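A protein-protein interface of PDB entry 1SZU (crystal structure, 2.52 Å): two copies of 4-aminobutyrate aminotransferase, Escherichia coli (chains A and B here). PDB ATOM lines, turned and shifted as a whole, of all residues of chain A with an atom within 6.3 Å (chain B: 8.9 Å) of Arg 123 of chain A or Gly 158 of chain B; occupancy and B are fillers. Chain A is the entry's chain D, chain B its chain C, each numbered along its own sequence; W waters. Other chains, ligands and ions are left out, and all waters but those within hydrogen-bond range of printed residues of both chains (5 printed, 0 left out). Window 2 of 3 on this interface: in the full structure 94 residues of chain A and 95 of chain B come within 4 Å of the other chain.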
ATOM      1  N   ALA A 118      38.010  -3.452   9.069  1.00  0.00           N
ATOM      2  CA  ALA A 118      38.017  -4.858   8.704  1.00  0.00           C
ATOM      3  C   ALA A 118      36.589  -5.437   8.802  1.00  0.00           C
ATOM      4  O   ALA A 118      36.123  -6.106   7.868  1.00  0.00           O
ATOM      5  CB  ALA A 118      38.962  -5.625   9.618  1.00  0.00           C
ATOM      6  N   VAL A 119      35.897  -5.173   9.921  1.00  0.00           N
ATOM      7  CA  VAL A 119      34.526  -5.656  10.129  1.00  0.00           C
ATOM      8  C   VAL A 119      33.551  -5.019   9.130  1.00  0.00           C
ATOM      9  O   VAL A 119      32.663  -5.695   8.605  1.00  0.00           O
ATOM     10  CB  VAL A 119      34.034  -5.365  11.574  1.00  0.00           C
ATOM     11  CG1 VAL A 119      32.536  -5.661  11.699  1.00  0.00           C
ATOM     12  CG2 VAL A 119      34.846  -6.205  12.598  1.00  0.00           C
ATOM     13  N   LYS A 120      33.714  -3.727   8.859  1.00  0.00           N
ATOM     14  CA  LYS A 120      32.856  -3.044   7.890  1.00  0.00           C
ATOM     15  C   LYS A 120      33.018  -3.696   6.503  1.00  0.00           C
ATOM     16  O   LYS A 120      32.047  -3.916   5.776  1.00  0.00           O
ATOM     17  CB  LYS A 120      33.242  -1.564   7.800  1.00  0.00           C
ATOM     18  CG  LYS A 120      32.544  -0.679   8.807  1.00  0.00           C
ATOM     19  CD  LYS A 120      33.298   0.656   8.997  1.00  0.00           C
ATOM     20  CE  LYS A 120      33.591   1.336   7.682  1.00  0.00           C
ATOM     21  NZ  LYS A 120      34.364   2.599   7.842  1.00  0.00           N
ATOM     22  N   ILE A 121      34.260  -3.992   6.144  1.00  0.00           N
ATOM     23  CA  ILE A 121      34.547  -4.618   4.870  1.00  0.00           C
ATOM     24  C   ILE A 121      33.971  -6.046   4.826  1.00  0.00           C
ATOM     25  O   ILE A 121      33.422  -6.458   3.795  1.00  0.00           O
ATOM     26  CB  ILE A 121      36.066  -4.644   4.605  1.00  0.00           C
ATOM     27  CG1 ILE A 121      36.561  -3.216   4.357  1.00  0.00           C
ATOM     28  CG2 ILE A 121      36.379  -5.542   3.409  1.00  0.00           C
ATOM     29  CD1 ILE A 121      38.079  -3.052   4.516  1.00  0.00           C
ATOM     30  N   ALA A 122      34.064  -6.794   5.930  1.00  0.00           N
ATOM     31  CA  ALA A 122      33.517  -8.143   5.916  1.00  0.00           C
ATOM     32  C   ALA A 122      32.005  -8.072   5.810  1.00  0.00           C
ATOM     33  O   ALA A 122      31.382  -8.914   5.168  1.00  0.00           O
ATOM     34  CB  ALA A 122      33.926  -8.916   7.147  1.00  0.00           C
ATOM     35  N   ARG A 123      31.408  -7.056   6.416  1.00  0.00           N
ATOM     36  CA  ARG A 123      29.960  -6.913   6.343  1.00  0.00           C
ATOM     37  C   ARG A 123      29.524  -6.603   4.923  1.00  0.00           C
ATOM     38  O   ARG A 123      28.537  -7.144   4.447  1.00  0.00           O
ATOM     39  CB  ARG A 123      29.477  -5.814   7.287  1.00  0.00           C
ATOM     40  CG  ARG A 123      29.625  -6.193   8.749  1.00  0.00           C
ATOM     41  CD  ARG A 123      29.263  -5.035   9.661  1.00  0.00           C
ATOM     42  NE  ARG A 123      27.882  -4.653   9.471  1.00  0.00           N
ATOM     43  CZ  ARG A 123      27.140  -4.054  10.393  1.00  0.00           C
ATOM     44  NH1 ARG A 123      27.658  -3.762  11.583  1.00  0.00           N
ATOM     45  NH2 ARG A 123      25.861  -3.777  10.133  1.00  0.00           N
ATOM     46  N   ALA A 124      30.265  -5.740   4.238  1.00  0.00           N
ATOM     47  CA  ALA A 124      29.925  -5.375   2.867  1.00  0.00           C
ATOM     48  C   ALA A 124      30.144  -6.555   1.900  1.00  0.00           C
ATOM     49  O   ALA A 124      29.399  -6.736   0.939  1.00  0.00           O
ATOM     50  CB  ALA A 124      30.763  -4.164   2.431  1.00  0.00           C
ATOM     51  N   ALA A 125      31.163  -7.368   2.168  1.00  0.00           N
ATOM     52  CA  ALA A 125      31.474  -8.492   1.307  1.00  0.00           C
ATOM     53  C   ALA A 125      30.510  -9.672   1.458  1.00  0.00           C
ATOM     54  O   ALA A 125      30.121 -10.293   0.475  1.00  0.00           O
ATOM     55  CB  ALA A 125      32.910  -8.959   1.572  1.00  0.00           C
ATOM     56  N   THR A 126      30.123  -9.984   2.690  1.00  0.00           N
ATOM     57  CA  THR A 126      29.246 -11.118   2.923  1.00  0.00           C
ATOM     58  C   THR A 126      27.804 -10.716   2.959  1.00  0.00           C
ATOM     59  O   THR A 126      26.923 -11.581   2.888  1.00  0.00           O
ATOM     60  CB  THR A 126      29.510 -11.767   4.269  1.00  0.00           C
ATOM     61  OG1 THR A 126      29.209 -10.808   5.298  1.00  0.00           O
ATOM     62  CG2 THR A 126      30.975 -12.244   4.376  1.00  0.00           C
ATOM     63  N   LYS A 127      27.564  -9.411   3.093  1.00  0.00           N
ATOM     64  CA  LYS A 127      26.203  -8.870   3.208  1.00  0.00           C
ATOM     65  C   LYS A 127      25.550  -9.366   4.509  1.00  0.00           C
ATOM     66  O   LYS A 127      24.354  -9.627   4.552  1.00  0.00           O
ATOM     67  CB  LYS A 127      25.346  -9.298   2.029  1.00  0.00           C
ATOM     68  CG  LYS A 127      25.915  -8.926   0.694  1.00  0.00           C
ATOM     69  CD  LYS A 127      25.379  -7.617   0.229  1.00  0.00           C
ATOM     70  CE  LYS A 127      25.660  -7.446  -1.246  1.00  0.00           C
ATOM     71  NZ  LYS A 127      25.024  -6.209  -1.794  1.00  0.00           N
ATOM     72  N   ARG A 128      26.350  -9.513   5.558  1.00  0.00           N
ATOM     73  CA  ARG A 128      25.855  -9.962   6.856  1.00  0.00           C
ATOM     74  C   ARG A 128      26.194  -8.892   7.886  1.00  0.00           C
ATOM     75  O   ARG A 128      27.071  -8.065   7.662  1.00  0.00           O
ATOM     76  CB  ARG A 128      26.516 -11.274   7.232  1.00  0.00           C
ATOM     77  CG  ARG A 128      26.211 -12.382   6.266  1.00  0.00           C
ATOM     78  CD  ARG A 128      27.046 -13.628   6.581  1.00  0.00           C
ATOM     79  NE  ARG A 128      26.873 -14.646   5.553  1.00  0.00           N
ATOM     80  CZ  ARG A 128      27.607 -15.751   5.442  1.00  0.00           C
ATOM     81  NH1 ARG A 128      28.590 -16.016   6.300  1.00  0.00           N
ATOM     82  NH2 ARG A 128      27.353 -16.595   4.453  1.00  0.00           N
ATOM     83  N   SER A 129      25.528  -8.919   9.030  1.00  0.00           N
ATOM     84  CA  SER A 129      25.763  -7.894  10.052  1.00  0.00           C
ATOM     85  C   SER A 129      26.414  -8.296  11.365  1.00  0.00           C
ATOM     86  O   SER A 129      26.935  -7.443  12.068  1.00  0.00           O
ATOM     87  CB  SER A 129      24.441  -7.201  10.380  1.00  0.00           C
ATOM     88  OG  SER A 129      23.985  -6.440   9.268  1.00  0.00           O
ATOM     89  N   GLY A 130      26.379  -9.578  11.698  1.00  0.00           N
ATOM     90  CA  GLY A 130      26.921 -10.025  12.967  1.00  0.00           C
ATOM     91  C   GLY A 130      28.375 -10.438  12.971  1.00  0.00           C
ATOM     92  O   GLY A 130      28.950 -10.793  11.935  1.00  0.00           O
ATOM     93  N   THR A 131      28.979 -10.369  14.152  1.00  0.00           N
ATOM     94  CA  THR A 131      30.359 -10.769  14.291  1.00  0.00           C
ATOM     95  C   THR A 131      30.478 -11.604  15.548  1.00  0.00           C
ATOM     96  O   THR A 131      29.627 -11.541  16.448  1.00  0.00           O
ATOM     97  CB  THR A 131      31.340  -9.541  14.377  1.00  0.00           C
ATOM     98  OG1 THR A 131      30.954  -8.682  15.456  1.00  0.00           O
ATOM     99  CG2 THR A 131      31.326  -8.737  13.079  1.00  0.00           C
ATOM    100  N   TYR A 144      32.056   0.071  19.008  1.00  0.00           N
ATOM    101  CA  TYR A 144      32.028  -1.255  18.420  1.00  0.00           C
ATOM    102  C   TYR A 144      33.181  -2.148  18.832  1.00  0.00           C
ATOM    103  O   TYR A 144      32.955  -3.323  19.138  1.00  0.00           O
ATOM    104  CB  TYR A 144      31.950  -1.171  16.897  1.00  0.00           C
ATOM    105  CG  TYR A 144      31.540  -2.487  16.287  1.00  0.00           C
ATOM    106  CD1 TYR A 144      30.192  -2.834  16.161  1.00  0.00           C
ATOM    107  CD2 TYR A 144      32.497  -3.405  15.881  1.00  0.00           C
ATOM    108  CE1 TYR A 144      29.806  -4.063  15.651  1.00  0.00           C
ATOM    109  CE2 TYR A 144      32.128  -4.650  15.363  1.00  0.00           C
ATOM    110  CZ  TYR A 144      30.783  -4.968  15.255  1.00  0.00           C
ATOM    111  OH  TYR A 144      30.430  -6.203  14.771  1.00  0.00           O
ATOM    112  N   ALA A 201      29.044 -12.150   9.530  1.00  0.00           N
ATOM    113  CA  ALA A 201      29.984 -11.646   8.519  1.00  0.00           C
ATOM    114  C   ALA A 201      31.419 -12.046   8.832  1.00  0.00           C
ATOM    115  O   ALA A 201      32.210 -12.309   7.934  1.00  0.00           O
ATOM    116  CB  ALA A 201      29.892 -10.110   8.442  1.00  0.00           C
ATOM    117  N   ALA A 202      31.748 -12.125  10.118  1.00  0.00           N
ATOM    118  CA  ALA A 202      33.115 -12.418  10.505  1.00  0.00           C
ATOM    119  C   ALA A 202      33.323 -12.965  11.918  1.00  0.00           C
ATOM    120  O   ALA A 202      32.478 -12.817  12.798  1.00  0.00           O
ATOM    121  CB  ALA A 202      33.937 -11.146  10.348  1.00  0.00           C
ATOM    122  N   MET A 235      34.039 -14.476   7.076  1.00  0.00           N
ATOM    123  CA  MET A 235      35.405 -13.963   6.960  1.00  0.00           C
ATOM    124  C   MET A 235      36.179 -14.158   8.271  1.00  0.00           C
ATOM    125  O   MET A 235      35.663 -13.883   9.363  1.00  0.00           O
ATOM    126  CB  MET A 235      35.378 -12.489   6.600  1.00  0.00           C
ATOM    127  CG  MET A 235      34.593 -12.185   5.347  1.00  0.00           C
ATOM    128  SD  MET A 235      35.386 -12.788   3.849  1.00  0.00           S
ATOM    129  CE  MET A 235      34.691 -14.446   3.693  1.00  0.00           C
ATOM    130  N   THR B 142      33.662   5.149  11.974  1.00  0.00           N
ATOM    131  CA  THR B 142      33.682   3.969  12.822  1.00  0.00           C
ATOM    132  C   THR B 142      32.216   3.582  12.833  1.00  0.00           C
ATOM    133  O   THR B 142      31.363   4.403  12.473  1.00  0.00           O
ATOM    134  CB  THR B 142      34.145   4.303  14.265  1.00  0.00           C
ATOM    135  OG1 THR B 142      33.319   5.342  14.808  1.00  0.00           O
ATOM    136  CG2 THR B 142      35.578   4.768  14.257  1.00  0.00           C
ATOM    137  N   HIS B 143      31.911   2.352  13.232  1.00  0.00           N
ATOM    138  CA  HIS B 143      30.512   1.943  13.248  1.00  0.00           C
ATOM    139  C   HIS B 143      29.638   3.002  13.924  1.00  0.00           C
ATOM    140  O   HIS B 143      28.696   3.531  13.312  1.00  0.00           O
ATOM    141  CB  HIS B 143      30.322   0.603  13.969  1.00  0.00           C
ATOM    142  CG  HIS B 143      30.547  -0.598  13.100  1.00  0.00           C
ATOM    143  ND1 HIS B 143      31.803  -1.079  12.801  1.00  0.00           N
ATOM    144  CD2 HIS B 143      29.670  -1.428  12.483  1.00  0.00           C
ATOM    145  CE1 HIS B 143      31.691  -2.154  12.041  1.00  0.00           C
ATOM    146  NE2 HIS B 143      30.407  -2.389  11.836  1.00  0.00           N
ATOM    147  N   TYR B 144      29.962   3.340  15.173  1.00  0.00           N
ATOM    148  CA  TYR B 144      29.145   4.309  15.901  1.00  0.00           C
ATOM    149  C   TYR B 144      29.140   5.723  15.312  1.00  0.00           C
ATOM    150  O   TYR B 144      28.090   6.362  15.294  1.00  0.00           O
ATOM    151  CB  TYR B 144      29.537   4.363  17.383  1.00  0.00           C
ATOM    152  CG  TYR B 144      28.475   5.029  18.225  1.00  0.00           C
ATOM    153  CD1 TYR B 144      27.387   4.298  18.728  1.00  0.00           C
ATOM    154  CD2 TYR B 144      28.536   6.399  18.495  1.00  0.00           C
ATOM    155  CE1 TYR B 144      26.381   4.922  19.483  1.00  0.00           C
ATOM    156  CE2 TYR B 144      27.542   7.033  19.250  1.00  0.00           C
ATOM    157  CZ  TYR B 144      26.470   6.295  19.738  1.00  0.00           C
ATOM    158  OH  TYR B 144      25.488   6.942  20.451  1.00  0.00           O
ATOM    159  N   LEU B 146      29.422   6.397  12.258  1.00  0.00           N
ATOM    160  CA  LEU B 146      28.679   6.301  10.991  1.00  0.00           C
ATOM    161  C   LEU B 146      27.183   6.388  11.341  1.00  0.00           C
ATOM    162  O   LEU B 146      26.397   6.914  10.556  1.00  0.00           O
ATOM    163  CB  LEU B 146      28.981   4.995  10.221  1.00  0.00           C
ATOM    164  CG  LEU B 146      30.318   4.982   9.440  1.00  0.00           C
ATOM    165  CD1 LEU B 146      30.595   3.601   8.895  1.00  0.00           C
ATOM    166  CD2 LEU B 146      30.286   5.974   8.287  1.00  0.00           C
ATOM    167  N   VAL B 152      24.082   7.908   4.662  1.00  0.00           N
ATOM    168  CA  VAL B 152      24.343   6.486   4.501  1.00  0.00           C
ATOM    169  C   VAL B 152      25.322   6.226   3.374  1.00  0.00           C
ATOM    170  O   VAL B 152      26.411   5.723   3.605  1.00  0.00           O
ATOM    171  CB  VAL B 152      23.027   5.714   4.243  1.00  0.00           C
ATOM    172  CG1 VAL B 152      23.321   4.324   3.759  1.00  0.00           C
ATOM    173  CG2 VAL B 152      22.218   5.646   5.514  1.00  0.00           C
ATOM    174  N   ASN B 153      24.956   6.572   2.151  1.00  0.00           N
ATOM    175  CA  ASN B 153      25.864   6.322   1.042  1.00  0.00           C
ATOM    176  C   ASN B 153      26.783   7.505   0.784  1.00  0.00           C
ATOM    177  O   ASN B 153      26.334   8.652   0.737  1.00  0.00           O
ATOM    178  CB  ASN B 153      25.073   5.956  -0.222  1.00  0.00           C
ATOM    179  CG  ASN B 153      25.860   6.213  -1.506  1.00  0.00           C
ATOM    180  OD1 ASN B 153      25.660   7.233  -2.169  1.00  0.00           O
ATOM    181  ND2 ASN B 153      26.769   5.296  -1.852  1.00  0.00           N
ATOM    182  N   PRO B 154      28.085   7.239   0.580  1.00  0.00           N
ATOM    183  CA  PRO B 154      28.716   5.916   0.573  1.00  0.00           C
ATOM    184  C   PRO B 154      29.331   5.516   1.905  1.00  0.00           C
ATOM    185  O   PRO B 154      29.662   4.349   2.099  1.00  0.00           O
ATOM    186  CB  PRO B 154      29.786   6.071  -0.493  1.00  0.00           C
ATOM    187  CG  PRO B 154      30.318   7.445  -0.164  1.00  0.00           C
ATOM    188  CD  PRO B 154      29.072   8.274   0.208  1.00  0.00           C
ATOM    189  N   TYR B 155      29.490   6.488   2.803  1.00  0.00           N
ATOM    190  CA  TYR B 155      30.096   6.270   4.117  1.00  0.00           C
ATOM    191  C   TYR B 155      29.788   4.924   4.757  1.00  0.00           C
ATOM    192  O   TYR B 155      30.689   4.299   5.297  1.00  0.00           O
ATOM    193  CB  TYR B 155      29.696   7.376   5.079  1.00  0.00           C
ATOM    194  CG  TYR B 155      30.051   8.761   4.612  1.00  0.00           C
ATOM    195  CD1 TYR B 155      29.138   9.797   4.738  1.00  0.00           C
ATOM    196  CD2 TYR B 155      31.276   9.033   4.019  1.00  0.00           C
ATOM    197  CE1 TYR B 155      29.422  11.068   4.284  1.00  0.00           C
ATOM    198  CE2 TYR B 155      31.580  10.310   3.554  1.00  0.00           C
ATOM    199  CZ  TYR B 155      30.644  11.326   3.685  1.00  0.00           C
ATOM    200  OH  TYR B 155      30.884  12.601   3.192  1.00  0.00           O
ATOM    201  N   SER B 156      28.540   4.469   4.712  1.00  0.00           N
ATOM    202  CA  SER B 156      28.204   3.164   5.310  1.00  0.00           C
ATOM    203  C   SER B 156      27.226   2.335   4.492  1.00  0.00           C
ATOM    204  O   SER B 156      26.355   1.671   5.058  1.00  0.00           O
ATOM    205  CB  SER B 156      27.636   3.335   6.745  1.00  0.00           C
ATOM    206  OG  SER B 156      26.457   4.129   6.788  1.00  0.00           O
ATOM    207  N   ALA B 157      27.388   2.366   3.171  1.00  0.00           N
ATOM    208  CA  ALA B 157      26.504   1.645   2.249  1.00  0.00           C
ATOM    209  C   ALA B 157      26.923   0.211   1.965  1.00  0.00           C
ATOM    210  O   ALA B 157      28.114  -0.082   1.838  1.00  0.00           O
ATOM    211  CB  ALA B 157      26.392   2.421   0.938  1.00  0.00           C
ATOM    212  N   GLY B 158      25.938  -0.675   1.849  1.00  0.00           N
ATOM    213  CA  GLY B 158      26.200  -2.085   1.584  1.00  0.00           C
ATOM    214  C   GLY B 158      26.567  -2.884   2.827  1.00  0.00           C
ATOM    215  O   GLY B 158      26.520  -4.119   2.837  1.00  0.00           O
ATOM    216  N   MET B 159      26.885  -2.174   3.903  1.00  0.00           N
ATOM    217  CA  MET B 159      27.321  -2.807   5.140  1.00  0.00           C
ATOM    218  C   MET B 159      26.242  -3.280   6.095  1.00  0.00           C
ATOM    219  O   MET B 159      26.533  -3.992   7.057  1.00  0.00           O
ATOM    220  CB  MET B 159      28.250  -1.848   5.880  1.00  0.00           C
ATOM    221  CG  MET B 159      29.475  -1.443   5.091  1.00  0.00           C
ATOM    222  SD  MET B 159      30.289  -0.120   5.908  1.00  0.00           S
ATOM    223  CE  MET B 159      30.621   1.084   4.594  1.00  0.00           C
ATOM    224  N   GLY B 160      24.998  -2.909   5.825  1.00  0.00           N
ATOM    225  CA  GLY B 160      23.917  -3.281   6.716  1.00  0.00           C
ATOM    226  C   GLY B 160      23.610  -2.089   7.609  1.00  0.00           C
ATOM    227  O   GLY B 160      24.143  -0.990   7.395  1.00  0.00           O
ATOM    228  N   LEU B 161      22.761  -2.282   8.610  1.00  0.00           N
ATOM    229  CA  LEU B 161      22.405  -1.177   9.507  1.00  0.00           C
ATOM    230  C   LEU B 161      23.435  -0.939  10.616  1.00  0.00           C
ATOM    231  O   LEU B 161      23.888  -1.875  11.305  1.00  0.00           O
ATOM    232  CB  LEU B 161      21.026  -1.421  10.123  1.00  0.00           C
ATOM    233  CG  LEU B 161      19.909  -1.439   9.075  1.00  0.00           C
ATOM    234  CD1 LEU B 161      18.590  -1.853   9.732  1.00  0.00           C
ATOM    235  CD2 LEU B 161      19.806  -0.072   8.395  1.00  0.00           C
ATOM    236  N   MET B 162      23.799   0.326  10.771  1.00  0.00           N
ATOM    237  CA  MET B 162      24.751   0.733  11.777  1.00  0.00           C
ATOM    238  C   MET B 162      24.110   0.720  13.182  1.00  0.00           C
ATOM    239  O   MET B 162      22.876   0.718  13.316  1.00  0.00           O
ATOM    240  CB  MET B 162      25.268   2.129  11.420  1.00  0.00           C
ATOM    241  CG  MET B 162      26.143   2.147  10.179  1.00  0.00           C
ATOM    242  SD  MET B 162      27.718   1.274  10.443  1.00  0.00           S
ATOM    243  CE  MET B 162      27.479  -0.284   9.589  1.00  0.00           C
ATOM    244  N   PRO B 163      24.939   0.708  14.241  1.00  0.00           N
ATOM    245  CA  PRO B 163      24.504   0.699  15.646  1.00  0.00           C
ATOM    246  C   PRO B 163      23.284   1.557  15.898  1.00  0.00           C
ATOM    247  O   PRO B 163      23.225   2.723  15.484  1.00  0.00           O
ATOM    248  CB  PRO B 163      25.716   1.225  16.378  1.00  0.00           C
ATOM    249  CG  PRO B 163      26.812   0.541  15.632  1.00  0.00           C
ATOM    250  CD  PRO B 163      26.408   0.775  14.169  1.00  0.00           C
ATOM    251  N   GLY B 164      22.305   0.974  16.577  1.00  0.00           N
ATOM    252  CA  GLY B 164      21.095   1.712  16.859  1.00  0.00           C
ATOM    253  C   GLY B 164      21.227   2.658  18.039  1.00  0.00           C
ATOM    254  O   GLY B 164      22.320   2.873  18.590  1.00  0.00           O
HETATM  255  O   HOH W   1      33.056   4.034   6.195  1.00  0.00           O
HETATM  256  O   HOH W   2      32.084   2.068  17.026  1.00  0.00           O
HETATM  257  O   HOH W   3      21.182  -5.045   8.786  1.00  0.00           O
HETATM  258  O   HOH W   4      25.849  -2.168  13.392  1.00  0.00           O
HETATM  259  O   HOH W   5      27.418  -5.152   0.077  1.00  0.00           O
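Among the printed residues, pairs that only touch across the chains: Val 119 of chain A with His 143 of chain B (3.6 Å), Ala 124 of chain A with Gly 158 of chain B (3.6 Å), Lys 120 of chain A with Met 159 of chain B (3.6 Å), Lys 120 of chain A with His 143 of chain B (3.7 Å), Tyr 144 of chain A with His 143 of chain B (3.8 Å), Arg 123 of chain A with Gly 160 of chain B (3.8 Å), Arg 123 of chain A with Met 162 of chain B (3.9 Å), Lys 120 of chain A with Leu 146 of chain B (3.9 Å) and Arg 123 of chain A with Gly 158 of chain B (3.98 Å).
Hydrophobic or aromatic side chains of chain B within 4 Å of the printed part of chain A: His 143, Leu 146, Met 159 and Met 162.
Hydrophobic or aromatic side chains of chain A that line the printed part of chain B: Val 119 and Tyr 144.
Among the printed residues, 12 pairs touch across the chains.
NE2 of His 143 of chain B is in hydrogen-bond range of NH1 of Arg 123 of chain A, 3.1 Å away.
The backbone carbonyl oxygen of Met 159 of chain B sits at hydrogen-bond distance from the guanidinium group of Arg 123 of chain A, at 2.8 Å.
The backbone carbonyl oxygen (O) of Leu 161 of chain B is in hydrogen-bond range of the guanidinium group (NH2) of Arg 123 of chain A.
Position printed for both chains: 144.
O of Arg 123 of chain A is in hydrogen-bond range of N of Arg 128 of chain A (3.4 Å).
NH2 of Arg 123 of chain A sits at hydrogen-bond distance from OG of Ser 129 of chain A.
The side-chain hydroxyl of Thr 131 of chain A sits at hydrogen-bond distance from the side-chain hydroxyl of Tyr 144 of chain A (2.6 Å).
Arg 123 of chain A touches just these residues of chain B: His 143 (3.1 Å), Gly 158 (3.98 Å), Met 159 (2.8 Å), Gly 160 (3.8 Å), Leu 161 (3.0 Å) and Met 162 (3.9 Å).
Of chain A, only Arg 123 (3.98 Å) and Ala 124 (3.6 Å) come within 4 Å of Gly 158 of chain B.
No residue of chain B comes within 4 Å of Ala 122 of chain A.
Of the printed residues of chain A, Met 159 of chain B touches Lys 120 (3.6 Å) and Arg 123 (2.8 Å).
Of the printed residues of chain B, Ala 124 of chain A touches Gly 158.
Of the printed residues of chain A, Leu 146 of chain B touches Lys 120 (3.9 Å).
Printed residues of chain A within 4 Å of His 143 of chain B: Val 119, Lys 120, Arg 123 and Tyr 144.
The nearest residue of chain B that does not touch Arg 123 of chain A is Pro 163 of chain B (5.4 Å).
The nearest residue of chain A that does not touch Gly 158 of chain B is Lys 127 of chain A (4.5 Å).
The nearest printed residue of chain A that does not touch Met 162 of chain B is Lys 120 of chain A (5.1 Å).
Water W1 lies within hydrogen-bond range of the side-chain amino group of Lys 120 of chain A (2.5 Å) and the backbone carbonyl oxygen of Tyr 155 of chain B (2.5 Å).
Water W5 lies within hydrogen-bond range of the backbone carbonyl oxygen (O) of Ala 124 of chain A (2.7 Å), the backbone carbonyl oxygen (O) of Gly 158 of chain B (3.1 Å) and the side-chain amino group (NZ) of Lys 127 of chain A (3.2 Å).
Water W2 bridges N of Tyr 144 of chain A (2.8 Å) and N of Tyr 144 of chain B (3.1 Å).
Water W4 lies within hydrogen-bond range of the backbone carbonyl oxygen of Leu 161 of chain B and the guanidinium group of Arg 123 of chain A.
Water W3 bridges OG of Ser 129 of chain A (3.2 Å) and N of Leu 161 of chain B (3.2 Å).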
